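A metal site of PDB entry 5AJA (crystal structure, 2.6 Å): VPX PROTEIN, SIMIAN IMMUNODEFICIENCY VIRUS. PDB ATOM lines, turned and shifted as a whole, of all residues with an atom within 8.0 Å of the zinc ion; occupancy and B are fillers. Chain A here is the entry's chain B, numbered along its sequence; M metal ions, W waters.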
ATOM      1  N   GLU A  34       8.152  29.248 -32.340  1.00  0.00           N
ATOM      2  CA  GLU A  34       8.996  28.065 -32.309  1.00  0.00           C
ATOM      3  C   GLU A  34      10.126  28.163 -31.290  1.00  0.00           C
ATOM      4  O   GLU A  34      10.380  27.209 -30.573  1.00  0.00           O
ATOM      5  CB  GLU A  34       9.592  27.809 -33.698  1.00  0.00           C
ATOM      6  CG  GLU A  34      10.390  26.539 -33.797  1.00  0.00           C
ATOM      7  CD  GLU A  34       9.551  25.303 -33.545  1.00  0.00           C
ATOM      8  OE1 GLU A  34       8.304  25.389 -33.661  1.00  0.00           O
ATOM      9  OE2 GLU A  34      10.138  24.258 -33.221  1.00  0.00           O
ATOM     10  N   ALA A  35      10.804  29.294 -31.217  1.00  0.00           N
ATOM     11  CA  ALA A  35      11.942  29.415 -30.320  1.00  0.00           C
ATOM     12  C   ALA A  35      11.529  29.245 -28.855  1.00  0.00           C
ATOM     13  O   ALA A  35      12.255  28.608 -28.086  1.00  0.00           O
ATOM     14  CB  ALA A  35      12.638  30.744 -30.526  1.00  0.00           C
ATOM     15  N   LEU A  37       9.622  27.329 -27.469  1.00  0.00           N
ATOM     16  CA  LEU A  37       9.580  25.920 -27.106  1.00  0.00           C
ATOM     17  C   LEU A  37      10.959  25.355 -26.792  1.00  0.00           C
ATOM     18  O   LEU A  37      11.062  24.238 -26.282  1.00  0.00           O
ATOM     19  CB  LEU A  37       8.966  25.077 -28.225  1.00  0.00           C
ATOM     20  CG  LEU A  37       7.653  25.489 -28.851  1.00  0.00           C
ATOM     21  CD1 LEU A  37       7.317  24.536 -29.992  1.00  0.00           C
ATOM     22  CD2 LEU A  37       6.547  25.515 -27.823  1.00  0.00           C
ATOM     23  N   HIS A  38      12.025  26.080 -27.116  1.00  0.00           N
ATOM     24  CA  HIS A  38      13.356  25.500 -27.023  1.00  0.00           C
ATOM     25  C   HIS A  38      14.279  26.309 -26.145  1.00  0.00           C
ATOM     26  O   HIS A  38      15.305  25.807 -25.688  1.00  0.00           O
ATOM     27  CB  HIS A  38      13.958  25.367 -28.425  1.00  0.00           C
ATOM     28  CG  HIS A  38      13.146  24.542 -29.358  1.00  0.00           C
ATOM     29  ND1 HIS A  38      12.992  23.182 -29.213  1.00  0.00           N
ATOM     30  CD2 HIS A  38      12.412  24.879 -30.450  1.00  0.00           C
ATOM     31  CE1 HIS A  38      12.215  22.713 -30.171  1.00  0.00           C
ATOM     32  NE2 HIS A  38      11.849  23.730 -30.933  1.00  0.00           N
ATOM     33  N   PHE A  39      13.924  27.565 -25.909  1.00  0.00           N
ATOM     34  CA  PHE A  39      14.812  28.480 -25.210  1.00  0.00           C
ATOM     35  C   PHE A  39      14.076  29.178 -24.093  1.00  0.00           C
ATOM     36  O   PHE A  39      12.853  29.364 -24.169  1.00  0.00           O
ATOM     37  CB  PHE A  39      15.400  29.523 -26.156  1.00  0.00           C
ATOM     38  CG  PHE A  39      16.164  28.940 -27.309  1.00  0.00           C
ATOM     39  CD1 PHE A  39      17.359  28.273 -27.090  1.00  0.00           C
ATOM     40  CD2 PHE A  39      15.713  29.074 -28.600  1.00  0.00           C
ATOM     41  CE1 PHE A  39      18.070  27.754 -28.143  1.00  0.00           C
ATOM     42  CE2 PHE A  39      16.427  28.551 -29.666  1.00  0.00           C
ATOM     43  CZ  PHE A  39      17.598  27.890 -29.446  1.00  0.00           C
ATOM     44  N   MET A  78      18.383  28.497 -33.631  1.00  0.00           N
ATOM     45  CA  MET A  78      17.519  27.336 -33.891  1.00  0.00           C
ATOM     46  C   MET A  78      18.285  26.217 -34.601  1.00  0.00           C
ATOM     47  O   MET A  78      18.109  25.041 -34.289  1.00  0.00           O
ATOM     48  CB  MET A  78      16.283  27.711 -34.723  1.00  0.00           C
ATOM     49  CG  MET A  78      15.179  28.425 -33.957  1.00  0.00           C
ATOM     50  SD  MET A  78      14.642  27.533 -32.467  1.00  0.00           S
ATOM     51  CE  MET A  78      14.347  25.884 -33.128  1.00  0.00           C
ATOM     52  N   HIS A  81      20.779  24.442 -32.057  1.00  0.00           N
ATOM     53  CA  HIS A  81      20.019  23.627 -31.126  1.00  0.00           C
ATOM     54  C   HIS A  81      19.506  22.325 -31.733  1.00  0.00           C
ATOM     55  O   HIS A  81      19.625  21.267 -31.122  1.00  0.00           O
ATOM     56  CB  HIS A  81      18.851  24.429 -30.578  1.00  0.00           C
ATOM     57  CG  HIS A  81      18.046  23.696 -29.557  1.00  0.00           C
ATOM     58  ND1 HIS A  81      18.362  23.714 -28.217  1.00  0.00           N
ATOM     59  CD2 HIS A  81      16.940  22.920 -29.673  1.00  0.00           C
ATOM     60  CE1 HIS A  81      17.482  22.990 -27.546  1.00  0.00           C
ATOM     61  NE2 HIS A  81      16.608  22.491 -28.412  1.00  0.00           N
ATOM     62  N   MET A  82      18.940  22.377 -32.939  1.00  0.00           N
ATOM     63  CA  MET A  82      18.356  21.172 -33.531  1.00  0.00           C
ATOM     64  C   MET A  82      19.426  20.206 -34.060  1.00  0.00           C
ATOM     65  O   MET A  82      19.217  18.997 -34.050  1.00  0.00           O
ATOM     66  CB  MET A  82      17.373  21.529 -34.641  1.00  0.00           C
ATOM     67  CG  MET A  82      16.282  22.494 -34.205  1.00  0.00           C
ATOM     68  SD  MET A  82      14.930  21.745 -33.283  1.00  0.00           S
ATOM     69  CE  MET A  82      14.436  20.478 -34.456  1.00  0.00           C
ATOM     70  N   GLY A  85      20.441  18.082 -31.135  1.00  0.00           N
ATOM     71  CA  GLY A  85      19.496  17.071 -30.735  1.00  0.00           C
ATOM     72  C   GLY A  85      18.452  17.608 -29.776  1.00  0.00           C
ATOM     73  O   GLY A  85      18.756  17.969 -28.636  1.00  0.00           O
ATOM     74  N   CYS A  86      17.223  17.641 -30.246  1.00  0.00           N
ATOM     75  CA  CYS A  86      16.097  18.129 -29.469  1.00  0.00           C
ATOM     76  C   CYS A  86      15.449  16.983 -28.675  1.00  0.00           C
ATOM     77  O   CYS A  86      15.061  15.968 -29.264  1.00  0.00           O
ATOM     78  CB  CYS A  86      15.083  18.795 -30.405  1.00  0.00           C
ATOM     79  SG  CYS A  86      13.746  19.711 -29.623  1.00  0.00           S
ATOM     80  N   PRO A  87      15.358  17.124 -27.342  1.00  0.00           N
ATOM     81  CA  PRO A  87      14.619  16.169 -26.507  1.00  0.00           C
ATOM     82  C   PRO A  87      13.193  15.910 -27.008  1.00  0.00           C
ATOM     83  O   PRO A  87      12.771  14.753 -27.068  1.00  0.00           O
ATOM     84  CB  PRO A  87      14.604  16.856 -25.139  1.00  0.00           C
ATOM     85  CG  PRO A  87      15.886  17.612 -25.107  1.00  0.00           C
ATOM     86  CD  PRO A  87      16.092  18.107 -26.520  1.00  0.00           C
ATOM     87  N   CYS A  88      12.472  16.969 -27.370  1.00  0.00           N
ATOM     88  CA  CYS A  88      11.123  16.850 -27.933  1.00  0.00           C
ATOM     89  C   CYS A  88      11.104  17.226 -29.415  1.00  0.00           C
ATOM     90  O   CYS A  88      10.614  16.468 -30.270  1.00  0.00           O
ATOM     91  CB  CYS A  88      10.138  17.725 -27.151  1.00  0.00           C
ATOM     92  SG  CYS A  88       9.967  17.330 -25.385  1.00  0.00           S
HETATM   93 ZN    ZN M   1      14.418  21.645 -28.265  1.00  0.00          ZN
HETATM   94  O   HOH W   1      13.997  21.814 -25.356  1.00  0.00           O
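SG of Cys 86 sits close to N of Cys 88 (3.8 Å).
NE2 of His 38 is in hydrogen-bond range of OE2 of Glu 34.
Three residues have an atom within 4 Å of the zinc ion: His 38, His 81 and Cys 86.
The nearest printed residue that does not touch the zinc ion is Pro 87 (4.3 Å).
ND1 of His 38 binds the zinc ion.
The zinc ion is bound by NE2 of His 81 (2.4 Å).
The zinc ion is bound by SG of Cys 86, 2.5 Å away.
The zinc ion has three donor atoms within binding distance.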
